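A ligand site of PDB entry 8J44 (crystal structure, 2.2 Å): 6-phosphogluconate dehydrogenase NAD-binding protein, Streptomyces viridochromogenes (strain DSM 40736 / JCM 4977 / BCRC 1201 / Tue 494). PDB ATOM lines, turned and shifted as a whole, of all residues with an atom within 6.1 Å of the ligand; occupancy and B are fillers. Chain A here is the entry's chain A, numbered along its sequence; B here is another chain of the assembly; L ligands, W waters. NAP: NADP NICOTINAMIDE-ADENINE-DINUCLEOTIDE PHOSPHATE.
The backbone carbonyl oxygen (O) of Thr 73 lies within hydrogen-bond range of an oxygen (O3D) of the ligand, at 3.2 Å. An oxygen (O3B) of the ligand lies within hydrogen-bond range of the backbone NH (N) of Gly 17, at 3.3 Å. The backbone carbonyl oxygen (O) of Val 72 is in hydrogen-bond range of an oxygen (O3D) of the ligand, 3.1 Å away. An oxygen (O4D) of the ligand is in hydrogen-bond range of the side-chain sulfur of Cys 71 (3.6 Å). The side-chain amino group (NZ) of Lys 43 is in salt-bridge range of an oxygen (O1X) of the ligand. The side-chain amide oxygen (OD1) of Asn 38 sits at hydrogen-bond distance from an oxygen (O3B) of the ligand (2.6 Å). The guanidinium group (NE) of Arg 39 is in salt-bridge range of an oxygen (O2X) of the ligand (3.1 Å). N of Thr 99 lies within hydrogen-bond range of O3D of the ligand, at 3.1 Å. The backbone NH of Leu 18 sits at hydrogen-bond distance from an oxygen (O1A) of the ligand (2.9 Å). N of Met 19 lies within hydrogen-bond range of O2N of the ligand. The side-chain carboxylate (OE2) of Glu 80 lies within hydrogen-bond range of a nitrogen (N6A) of the ligand. OG1 of Thr 40 sits at hydrogen-bond distance from O2X of the ligand (2.7 Å). The backbone NH (N) of Leu 16 is in hydrogen-bond range of an oxygen (O3B) of the ligand. The backbone NH of Thr 40 lies within hydrogen-bond range of an oxygen (O2X) of the ligand (2.9 Å). O4B of the ligand lies within hydrogen-bond range of N of Thr 73. The side-chain hydroxyl of Thr 99 sits close to an oxygen (O2D) of the ligand, at 3.5 Å. An oxygen (O4B) of the ligand sits close to the side-chain hydroxyl (OG1) of Thr 73 (3.5 Å).
Water W4 lies within hydrogen-bond range of O2N of the ligand (2.5 Å), N of Gly 17 (2.8 Å), N of Gly 20 (3.0 Å) and O of Cys 71 (3.1 Å). Water W2 lies within hydrogen-bond range of the side-chain hydroxyl of Thr 73 (2.5 Å) and an oxygen (O2A) of the ligand (2.7 Å). Water W3 lies within hydrogen-bond range of the side-chain amide oxygen of Asn 38 (2.8 Å), the backbone NH of Arg 39 (2.9 Å) and a nitrogen (N3A) of the ligand (3.0 Å).
CA of Gly 15 touches O3B of the ligand, at 3.8 Å. Gly 20 touches the ligand (N to O2N, 3.9 Å). CB of Ala 77 touches N7A of the ligand (3.6 Å). Leu 81 touches the ligand. CG2 of Thr 98 touches O3D of the ligand, at 3.8 Å. Ile 124 touches the ligand (O to C5N, 3.3 Å). Ala 126 touches the ligand. CA of Ile 127 touches O7N of the ligand, 3.9 Å away. Pro 128 touches the ligand. Hydrophobic or aromatic side chains within 4 Å of the ligand: Leu 18, Met 19, Val 72, Ala 77, Leu 81 and Pro 128. Of the 32 residues printed, 22 come within 4 Å of the ligand. The nearest printed residue that does not touch the ligand is Trp 37 (4.3 Å).
The backbone NH of Gly 15 lies within hydrogen-bond range of the backbone carbonyl oxygen of Trp 37, 3.0 Å away. ND2 of Asn 38 is in hydrogen-bond range of O of Thr 40. OG1 of Thr 98 sits at hydrogen-bond distance from N of Val 72, 3.2 Å away. The backbone carbonyl oxygen of Leu 16 sits close to the side-chain amide oxygen of Gln 21 (2.8 Å). The side-chain amide oxygen (OD1) of Asn 38 lies within hydrogen-bond range of the backbone NH (N) of Leu 16 (2.9 Å). The side-chain carboxylate (OD1) of Asp 74 is in hydrogen-bond range of the backbone NH (N) of Ala 77, 2.8 Å away.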
ATOM      1  N   GLY A  15      14.163   6.794  30.218  1.00  0.00           N
ATOM      2  CA  GLY A  15      14.187   8.190  29.785  1.00  0.00           C
ATOM      3  C   GLY A  15      12.767   8.722  29.521  1.00  0.00           C
ATOM      4  O   GLY A  15      12.145   8.412  28.496  1.00  0.00           O
ATOM      5  N   LEU A  16      12.275   9.564  30.425  1.00  0.00           N
ATOM      6  CA  LEU A  16      10.942  10.126  30.281  1.00  0.00           C
ATOM      7  C   LEU A  16      10.927  11.633  30.133  1.00  0.00           C
ATOM      8  O   LEU A  16      10.188  12.311  30.838  1.00  0.00           O
ATOM      9  CB  LEU A  16      10.105   9.707  31.502  1.00  0.00           C
ATOM     10  CG  LEU A  16      10.002   8.200  31.738  1.00  0.00           C
ATOM     11  CD1 LEU A  16       9.228   7.934  33.007  1.00  0.00           C
ATOM     12  CD2 LEU A  16       9.335   7.511  30.548  1.00  0.00           C
ATOM     13  N   GLY A  17      11.736  12.156  29.212  1.00  0.00           N
ATOM     14  CA  GLY A  17      11.676  13.578  28.870  1.00  0.00           C
ATOM     15  C   GLY A  17      10.464  13.845  28.009  1.00  0.00           C
ATOM     16  O   GLY A  17       9.574  12.987  27.900  1.00  0.00           O
ATOM     17  N   LEU A  18      10.430  14.981  27.355  1.00  0.00           N
ATOM     18  CA  LEU A  18       9.276  15.281  26.497  1.00  0.00           C
ATOM     19  C   LEU A  18       9.000  14.166  25.472  1.00  0.00           C
ATOM     20  O   LEU A  18       7.840  13.786  25.267  1.00  0.00           O
ATOM     21  CB  LEU A  18       9.457  16.644  25.811  1.00  0.00           C
ATOM     22  CG  LEU A  18       9.316  17.805  26.822  1.00  0.00           C
ATOM     23  CD1 LEU A  18       9.801  19.168  26.293  1.00  0.00           C
ATOM     24  CD2 LEU A  18       7.874  17.868  27.311  1.00  0.00           C
ATOM     25  N   MET A  19      10.037  13.649  24.842  1.00  0.00           N
ATOM     26  CA  MET A  19       9.858  12.613  23.825  1.00  0.00           C
ATOM     27  C   MET A  19       9.612  11.233  24.456  1.00  0.00           C
ATOM     28  O   MET A  19       8.692  10.532  24.078  1.00  0.00           O
ATOM     29  CB  MET A  19      11.037  12.582  22.852  1.00  0.00           C
ATOM     30  CG  MET A  19      10.936  11.478  21.806  1.00  0.00           C
ATOM     31  SD  MET A  19       9.411  11.558  20.843  1.00  0.00           S
ATOM     32  CE  MET A  19       9.740  12.960  19.739  1.00  0.00           C
ATOM     33  N   GLY A  20      10.437  10.875  25.440  1.00  0.00           N
ATOM     34  CA  GLY A  20      10.281   9.606  26.161  1.00  0.00           C
ATOM     35  C   GLY A  20       8.875   9.403  26.729  1.00  0.00           C
ATOM     36  O   GLY A  20       8.335   8.277  26.687  1.00  0.00           O
ATOM     37  N   GLN A  21       8.308  10.479  27.274  1.00  0.00           N
ATOM     38  CA  GLN A  21       6.946  10.404  27.855  1.00  0.00           C
ATOM     39  C   GLN A  21       5.936  10.021  26.773  1.00  0.00           C
ATOM     40  O   GLN A  21       5.075   9.204  27.026  1.00  0.00           O
ATOM     41  CB  GLN A  21       6.517  11.730  28.516  1.00  0.00           C
ATOM     42  CG  GLN A  21       7.106  11.895  29.917  1.00  0.00           C
ATOM     43  CD  GLN A  21       6.908  13.288  30.506  1.00  0.00           C
ATOM     44  OE1 GLN A  21       7.853  13.937  30.935  1.00  0.00           O
ATOM     45  NE2 GLN A  21       5.679  13.747  30.517  1.00  0.00           N
ATOM     46  N   TRP A  37      11.203   4.218  33.675  1.00  0.00           N
ATOM     47  CA  TRP A  37      12.219   4.689  34.613  1.00  0.00           C
ATOM     48  C   TRP A  37      12.738   6.005  34.106  1.00  0.00           C
ATOM     49  O   TRP A  37      12.983   6.181  32.926  1.00  0.00           O
ATOM     50  CB  TRP A  37      13.353   3.681  34.764  1.00  0.00           C
ATOM     51  CG  TRP A  37      14.388   4.142  35.762  1.00  0.00           C
ATOM     52  CD1 TRP A  37      14.391   3.883  37.087  1.00  0.00           C
ATOM     53  CD2 TRP A  37      15.548   4.969  35.521  1.00  0.00           C
ATOM     54  NE1 TRP A  37      15.464   4.485  37.704  1.00  0.00           N
ATOM     55  CE2 TRP A  37      16.192   5.162  36.760  1.00  0.00           C
ATOM     56  CE3 TRP A  37      16.093   5.571  34.375  1.00  0.00           C
ATOM     57  CZ2 TRP A  37      17.371   5.918  36.906  1.00  0.00           C
ATOM     58  CZ3 TRP A  37      17.249   6.342  34.504  1.00  0.00           C
ATOM     59  CH2 TRP A  37      17.880   6.508  35.766  1.00  0.00           C
ATOM     60  N   ASN A  38      12.864   6.952  35.021  1.00  0.00           N
ATOM     61  CA  ASN A  38      13.528   8.224  34.767  1.00  0.00           C
ATOM     62  C   ASN A  38      14.443   8.592  35.942  1.00  0.00           C
ATOM     63  O   ASN A  38      14.133   8.252  37.083  1.00  0.00           O
ATOM     64  CB  ASN A  38      12.509   9.318  34.490  1.00  0.00           C
ATOM     65  CG  ASN A  38      13.132  10.532  33.861  1.00  0.00           C
ATOM     66  OD1 ASN A  38      13.709  10.466  32.758  1.00  0.00           O
ATOM     67  ND2 ASN A  38      13.040  11.672  34.543  1.00  0.00           N
ATOM     68  N   ARG A  39      15.540   9.278  35.646  1.00  0.00           N
ATOM     69  CA  ARG A  39      16.442   9.748  36.695  1.00  0.00           C
ATOM     70  C   ARG A  39      15.690  10.642  37.712  1.00  0.00           C
ATOM     71  O   ARG A  39      15.689  10.369  38.896  1.00  0.00           O
ATOM     72  CB  ARG A  39      17.653  10.464  36.049  1.00  0.00           C
ATOM     73  CG  ARG A  39      18.521  11.307  36.972  1.00  0.00           C
ATOM     74  CD  ARG A  39      19.700  11.869  36.181  1.00  0.00           C
ATOM     75  NE  ARG A  39      19.275  12.851  35.200  1.00  0.00           N
ATOM     76  CZ  ARG A  39      20.092  13.607  34.471  1.00  0.00           C
ATOM     77  NH1 ARG A  39      21.417  13.478  34.585  1.00  0.00           N
ATOM     78  NH2 ARG A  39      19.589  14.477  33.593  1.00  0.00           N
ATOM     79  N   THR A  40      15.004  11.678  37.222  1.00  0.00           N
ATOM     80  CA  THR A  40      14.102  12.487  38.049  1.00  0.00           C
ATOM     81  C   THR A  40      12.770  11.738  38.180  1.00  0.00           C
ATOM     82  O   THR A  40      11.965  11.718  37.229  1.00  0.00           O
ATOM     83  CB  THR A  40      13.836  13.859  37.428  1.00  0.00           C
ATOM     84  OG1 THR A  40      15.070  14.459  37.045  1.00  0.00           O
ATOM     85  CG2 THR A  40      13.108  14.772  38.424  1.00  0.00           C
ATOM     86  N   ALA A  41      12.546  11.107  39.322  1.00  0.00           N
ATOM     87  CA  ALA A  41      11.484  10.123  39.510  1.00  0.00           C
ATOM     88  C   ALA A  41      10.043  10.660  39.286  1.00  0.00           C
ATOM     89  O   ALA A  41       9.156   9.922  38.872  1.00  0.00           O
ATOM     90  CB  ALA A  41      11.591   9.513  40.888  1.00  0.00           C
ATOM     91  N   LYS A  43       8.874  12.642  37.056  1.00  0.00           N
ATOM     92  CA  LYS A  43       8.422  12.723  35.643  1.00  0.00           C
ATOM     93  C   LYS A  43       7.648  11.478  35.198  1.00  0.00           C
ATOM     94  O   LYS A  43       6.914  11.528  34.219  1.00  0.00           O
ATOM     95  CB  LYS A  43       9.603  12.999  34.746  1.00  0.00           C
ATOM     96  CG  LYS A  43      10.242  14.344  35.004  1.00  0.00           C
ATOM     97  CD  LYS A  43      11.089  14.758  33.813  1.00  0.00           C
ATOM     98  CE  LYS A  43      11.960  15.990  34.089  1.00  0.00           C
ATOM     99  NZ  LYS A  43      12.821  16.198  32.892  1.00  0.00           N
ATOM    100  N   CYS A  71      15.662   6.655  25.446  1.00  0.00           N
ATOM    101  CA  CYS A  71      15.456   7.923  24.805  1.00  0.00           C
ATOM    102  C   CYS A  71      15.853   8.976  25.791  1.00  0.00           C
ATOM    103  O   CYS A  71      15.033   9.446  26.588  1.00  0.00           O
ATOM    104  CB  CYS A  71      14.003   8.093  24.325  1.00  0.00           C
ATOM    105  SG  CYS A  71      13.762   9.618  23.348  1.00  0.00           S
ATOM    106  N   VAL A  72      17.147   9.314  25.741  1.00  0.00           N
ATOM    107  CA  VAL A  72      17.767  10.281  26.635  1.00  0.00           C
ATOM    108  C   VAL A  72      18.494  11.403  25.839  1.00  0.00           C
ATOM    109  O   VAL A  72      18.480  11.441  24.592  1.00  0.00           O
ATOM    110  CB  VAL A  72      18.685   9.578  27.655  1.00  0.00           C
ATOM    111  CG1 VAL A  72      17.884   8.620  28.542  1.00  0.00           C
ATOM    112  CG2 VAL A  72      19.830   8.824  26.960  1.00  0.00           C
ATOM    113  N   THR A  73      19.119  12.336  26.566  1.00  0.00           N
ATOM    114  CA  THR A  73      19.721  13.516  25.923  1.00  0.00           C
ATOM    115  C   THR A  73      20.762  13.174  24.848  1.00  0.00           C
ATOM    116  O   THR A  73      20.656  13.684  23.730  1.00  0.00           O
ATOM    117  CB  THR A  73      20.356  14.465  26.977  1.00  0.00           C
ATOM    118  OG1 THR A  73      19.380  14.831  27.970  1.00  0.00           O
ATOM    119  CG2 THR A  73      20.881  15.769  26.272  1.00  0.00           C
ATOM    120  N   ASP A  74      21.716  12.311  25.174  1.00  0.00           N
ATOM    121  CA  ASP A  74      22.835  11.994  24.261  1.00  0.00           C
ATOM    122  C   ASP A  74      23.461  10.627  24.565  1.00  0.00           C
ATOM    123  O   ASP A  74      23.078   9.965  25.531  1.00  0.00           O
ATOM    124  CB  ASP A  74      23.925  13.102  24.320  1.00  0.00           C
ATOM    125  CG  ASP A  74      24.465  13.350  25.737  1.00  0.00           C
ATOM    126  OD1 ASP A  74      24.603  12.405  26.566  1.00  0.00           O
ATOM    127  OD2 ASP A  74      24.740  14.523  26.007  1.00  0.00           O
ATOM    128  N   GLY A  76      26.505   9.924  25.539  1.00  0.00           N
ATOM    129  CA  GLY A  76      27.118   9.971  26.875  1.00  0.00           C
ATOM    130  C   GLY A  76      26.189   9.465  27.969  1.00  0.00           C
ATOM    131  O   GLY A  76      26.551   8.557  28.758  1.00  0.00           O
ATOM    132  N   ALA A  77      24.960   9.983  27.966  1.00  0.00           N
ATOM    133  CA  ALA A  77      23.951   9.491  28.915  1.00  0.00           C
ATOM    134  C   ALA A  77      23.682   8.012  28.741  1.00  0.00           C
ATOM    135  O   ALA A  77      23.595   7.242  29.725  1.00  0.00           O
ATOM    136  CB  ALA A  77      22.673  10.296  28.786  1.00  0.00           C
ATOM    137  N   GLU A  80      26.684   5.878  30.171  1.00  0.00           N
ATOM    138  CA  GLU A  80      26.596   5.968  31.624  1.00  0.00           C
ATOM    139  C   GLU A  80      25.563   4.991  32.199  1.00  0.00           C
ATOM    140  O   GLU A  80      25.859   4.294  33.168  1.00  0.00           O
ATOM    141  CB  GLU A  80      26.301   7.410  32.007  1.00  0.00           C
ATOM    142  CG  GLU A  80      26.093   7.648  33.498  1.00  0.00           C
ATOM    143  CD  GLU A  80      25.785   9.107  33.771  1.00  0.00           C
ATOM    144  OE1 GLU A  80      26.569   9.958  33.328  1.00  0.00           O
ATOM    145  OE2 GLU A  80      24.725   9.406  34.349  1.00  0.00           O
ATOM    146  N   LEU A  81      24.387   4.900  31.571  1.00  0.00           N
ATOM    147  CA  LEU A  81      23.347   4.010  32.086  1.00  0.00           C
ATOM    148  C   LEU A  81      23.578   2.508  31.832  1.00  0.00           C
ATOM    149  O   LEU A  81      23.289   1.667  32.690  1.00  0.00           O
ATOM    150  CB  LEU A  81      22.000   4.418  31.484  1.00  0.00           C
ATOM    151  CG  LEU A  81      21.477   5.800  31.888  1.00  0.00           C
ATOM    152  CD1 LEU A  81      20.261   6.133  31.071  1.00  0.00           C
ATOM    153  CD2 LEU A  81      21.155   5.837  33.382  1.00  0.00           C
ATOM    154  N   LEU A  97      16.735   5.109  20.806  1.00  0.00           N
ATOM    155  CA  LEU A  97      16.163   6.201  20.014  1.00  0.00           C
ATOM    156  C   LEU A  97      16.684   7.549  20.425  1.00  0.00           C
ATOM    157  O   LEU A  97      16.117   8.567  20.040  1.00  0.00           O
ATOM    158  CB  LEU A  97      14.638   6.209  20.079  1.00  0.00           C
ATOM    159  CG  LEU A  97      13.986   4.981  19.437  1.00  0.00           C
ATOM    160  CD1 LEU A  97      12.529   4.795  19.856  1.00  0.00           C
ATOM    161  CD2 LEU A  97      14.069   5.112  17.939  1.00  0.00           C
ATOM    162  N   THR A  98      17.777   7.568  21.152  1.00  0.00           N
ATOM    163  CA  THR A  98      18.521   8.814  21.365  1.00  0.00           C
ATOM    164  C   THR A  98      19.090   9.306  20.019  1.00  0.00           C
ATOM    165  O   THR A  98      19.524   8.508  19.184  1.00  0.00           O
ATOM    166  CB  THR A  98      19.686   8.559  22.348  1.00  0.00           C
ATOM    167  OG1 THR A  98      19.163   7.993  23.571  1.00  0.00           O
ATOM    168  CG2 THR A  98      20.425   9.825  22.674  1.00  0.00           C
ATOM    169  N   THR A  99      19.060  10.614  19.812  1.00  0.00           N
ATOM    170  CA  THR A  99      19.670  11.255  18.640  1.00  0.00           C
ATOM    171  C   THR A  99      21.190  11.432  18.855  1.00  0.00           C
ATOM    172  O   THR A  99      21.643  11.790  19.946  1.00  0.00           O
ATOM    173  CB  THR A  99      18.996  12.608  18.361  1.00  0.00           C
ATOM    174  OG1 THR A  99      17.680  12.364  17.886  1.00  0.00           O
ATOM    175  CG2 THR A  99      19.770  13.470  17.339  1.00  0.00           C
ATOM    176  N   GLY A 100      21.962  11.134  17.808  1.00  0.00           N
ATOM    177  CA  GLY A 100      23.422  11.189  17.873  1.00  0.00           C
ATOM    178  C   GLY A 100      24.088  11.148  16.497  1.00  0.00           C
ATOM    179  O   GLY A 100      23.424  11.307  15.491  1.00  0.00           O
ATOM    180  N   ILE A 124      14.228   9.448  15.665  1.00  0.00           N
ATOM    181  CA  ILE A 124      12.823   9.869  15.635  1.00  0.00           C
ATOM    182  C   ILE A 124      12.651  11.129  14.755  1.00  0.00           C
ATOM    183  O   ILE A 124      13.222  12.169  15.045  1.00  0.00           O
ATOM    184  CB  ILE A 124      12.307  10.160  17.056  1.00  0.00           C
ATOM    185  CG1 ILE A 124      12.512   8.938  17.942  1.00  0.00           C
ATOM    186  CG2 ILE A 124      10.829  10.522  17.011  1.00  0.00           C
ATOM    187  CD1 ILE A 124      12.358   9.222  19.405  1.00  0.00           C
ATOM    188  N   MET A 125      11.875  10.998  13.690  1.00  0.00           N
ATOM    189  CA  MET A 125      11.564  12.110  12.763  1.00  0.00           C
ATOM    190  C   MET A 125      10.127  12.564  13.020  1.00  0.00           C
ATOM    191  O   MET A 125       9.214  12.308  12.255  1.00  0.00           O
ATOM    192  CB  MET A 125      11.679  11.585  11.314  1.00  0.00           C
ATOM    193  CG  MET A 125      12.998  10.882  10.994  1.00  0.00           C
ATOM    194  SD  MET A 125      14.451  11.883  11.405  1.00  0.00           S
ATOM    195  CE  MET A 125      14.061  13.471  10.651  1.00  0.00           C
ATOM    196  N   ALA A 126       9.929  13.209  14.156  1.00  0.00           N
ATOM    197  CA  ALA A 126       8.588  13.554  14.632  1.00  0.00           C
ATOM    198  C   ALA A 126       8.731  14.391  15.881  1.00  0.00           C
ATOM    199  O   ALA A 126       9.755  14.298  16.556  1.00  0.00           O
ATOM    200  CB  ALA A 126       7.793  12.302  14.929  1.00  0.00           C
ATOM    201  N   ILE A 127       7.722  15.206  16.161  1.00  0.00           N
ATOM    202  CA  ILE A 127       7.553  15.874  17.491  1.00  0.00           C
ATOM    203  C   ILE A 127       6.683  15.016  18.426  1.00  0.00           C
ATOM    204  O   ILE A 127       5.918  14.190  17.946  1.00  0.00           O
ATOM    205  CB  ILE A 127       6.934  17.280  17.362  1.00  0.00           C
ATOM    206  CG1 ILE A 127       5.614  17.248  16.587  1.00  0.00           C
ATOM    207  CG2 ILE A 127       7.935  18.240  16.700  1.00  0.00           C
ATOM    208  CD1 ILE A 127       4.789  18.526  16.702  1.00  0.00           C
ATOM    209  N   PRO A 128       6.798  15.216  19.744  1.00  0.00           N
ATOM    210  CA  PRO A 128       6.079  14.325  20.681  1.00  0.00           C
ATOM    211  C   PRO A 128       4.580  14.180  20.415  1.00  0.00           C
ATOM    212  O   PRO A 128       4.074  13.055  20.375  1.00  0.00           O
ATOM    213  CB  PRO A 128       6.386  14.942  22.060  1.00  0.00           C
ATOM    214  CG  PRO A 128       7.722  15.576  21.891  1.00  0.00           C
ATOM    215  CD  PRO A 128       7.719  16.112  20.466  1.00  0.00           C
ATOM    216  N   ASP B 238       6.262  22.780  18.961  1.00  0.00           N
ATOM    217  CA  ASP B 238       7.283  21.782  18.571  1.00  0.00           C
ATOM    218  C   ASP B 238       8.766  22.006  19.007  1.00  0.00           C
ATOM    219  O   ASP B 238       9.296  21.262  19.831  1.00  0.00           O
ATOM    220  CB  ASP B 238       7.202  21.501  17.022  1.00  0.00           C
ATOM    221  CG  ASP B 238       6.677  22.703  16.145  1.00  0.00           C
ATOM    222  OD1 ASP B 238       7.093  23.860  16.330  1.00  0.00           O
ATOM    223  OD2 ASP B 238       5.867  22.467  15.209  1.00  0.00           O
ATOM    224  N   ALA B 239       9.399  23.031  18.419  1.00  0.00           N
ATOM    225  CA  ALA B 239      10.846  23.152  18.369  1.00  0.00           C
ATOM    226  C   ALA B 239      11.288  24.608  18.233  1.00  0.00           C
ATOM    227  O   ALA B 239      10.852  25.320  17.336  1.00  0.00           O
ATOM    228  CB  ALA B 239      11.364  22.354  17.178  1.00  0.00           C
HETATM  229  PA  NAP L   1      14.422  16.131  27.365  1.00  0.00           P
HETATM  230  O1A NAP L   1      12.956  16.440  27.455  1.00  0.00           O
HETATM  231  O2A NAP L   1      15.537  17.108  27.669  1.00  0.00           O
HETATM  232  O5B NAP L   1      14.697  14.811  28.267  1.00  0.00           O
HETATM  233  C5B NAP L   1      16.026  14.261  28.318  1.00  0.00           C
HETATM  234  C4B NAP L   1      15.942  12.917  29.025  1.00  0.00           C
HETATM  235  O4B NAP L   1      17.258  12.367  29.160  1.00  0.00           O
HETATM  236  C3B NAP L   1      15.365  13.007  30.440  1.00  0.00           C
HETATM  237  O3B NAP L   1      14.639  11.818  30.793  1.00  0.00           O
HETATM  238  C2B NAP L   1      16.602  13.052  31.299  1.00  0.00           C
HETATM  239  O2B NAP L   1      16.338  12.651  32.650  1.00  0.00           O
HETATM  240  C1B NAP L   1      17.466  12.065  30.537  1.00  0.00           C
HETATM  241  N9A NAP L   1      18.928  12.139  30.836  1.00  0.00           N
HETATM  242  C8A NAP L   1      19.855  13.035  30.346  1.00  0.00           C
HETATM  243  N7A NAP L   1      21.096  12.734  30.834  1.00  0.00           N
HETATM  244  C5A NAP L   1      20.930  11.646  31.636  1.00  0.00           C
HETATM  245  C6A NAP L   1      21.792  10.792  32.466  1.00  0.00           C
HETATM  246  N6A NAP L   1      23.103  11.074  32.544  1.00  0.00           N
HETATM  247  N1A NAP L   1      21.273   9.715  33.134  1.00  0.00           N
HETATM  248  C2A NAP L   1      19.937   9.439  33.074  1.00  0.00           C
HETATM  249  N3A NAP L   1      19.098  10.206  32.319  1.00  0.00           N
HETATM  250  C4A NAP L   1      19.528  11.259  31.609  1.00  0.00           C
HETATM  251  O3  NAP L   1      14.711  15.690  25.852  1.00  0.00           O
HETATM  252  PN  NAP L   1      13.724  14.925  24.811  1.00  0.00           P
HETATM  253  O1N NAP L   1      13.010  15.843  23.888  1.00  0.00           O
HETATM  254  O2N NAP L   1      12.961  13.838  25.557  1.00  0.00           O
HETATM  255  O5D NAP L   1      14.860  14.242  23.886  1.00  0.00           O
HETATM  256  C5D NAP L   1      15.435  12.968  24.098  1.00  0.00           C
HETATM  257  C4D NAP L   1      16.053  12.535  22.778  1.00  0.00           C
HETATM  258  O4D NAP L   1      15.022  12.536  21.755  1.00  0.00           O
HETATM  259  C3D NAP L   1      17.128  13.512  22.315  1.00  0.00           C
HETATM  260  O3D NAP L   1      18.252  12.794  21.849  1.00  0.00           O
HETATM  261  C2D NAP L   1      16.427  14.280  21.208  1.00  0.00           C
HETATM  262  O2D NAP L   1      17.320  14.865  20.246  1.00  0.00           O
HETATM  263  C1D NAP L   1      15.478  13.225  20.614  1.00  0.00           C
HETATM  264  N1N NAP L   1      14.394  13.809  19.840  1.00  0.00           N
HETATM  265  C2N NAP L   1      13.547  14.681  20.444  1.00  0.00           C
HETATM  266  C3N NAP L   1      12.528  15.306  19.708  1.00  0.00           C
HETATM  267  C7N NAP L   1      11.563  16.297  20.310  1.00  0.00           C
HETATM  268  O7N NAP L   1      10.748  16.814  19.526  1.00  0.00           O
HETATM  269  N7N NAP L   1      11.592  16.593  21.610  1.00  0.00           N
HETATM  270  C4N NAP L   1      12.372  14.974  18.350  1.00  0.00           C
HETATM  271  C5N NAP L   1      13.247  14.071  17.766  1.00  0.00           C
HETATM  272  C6N NAP L   1      14.263  13.498  18.525  1.00  0.00           C
HETATM  273  P2B NAP L   1      15.849  13.789  33.674  1.00  0.00           P
HETATM  274  O1X NAP L   1      14.365  13.929  33.465  1.00  0.00           O
HETATM  275  O2X NAP L   1      16.188  13.172  34.989  1.00  0.00           O
HETATM  276  O3X NAP L   1      16.543  15.057  33.224  1.00  0.00           O
HETATM  277  O   HOH W   1      23.751  14.072  30.094  1.00  0.00           O
HETATM  278  O   HOH W   2      18.033  16.538  26.823  1.00  0.00           O
HETATM  279  O   HOH W   3      16.286   9.349  32.867  1.00  0.00           O
HETATM  280  O   HOH W   4      12.983  11.707  26.790  1.00  0.00           O
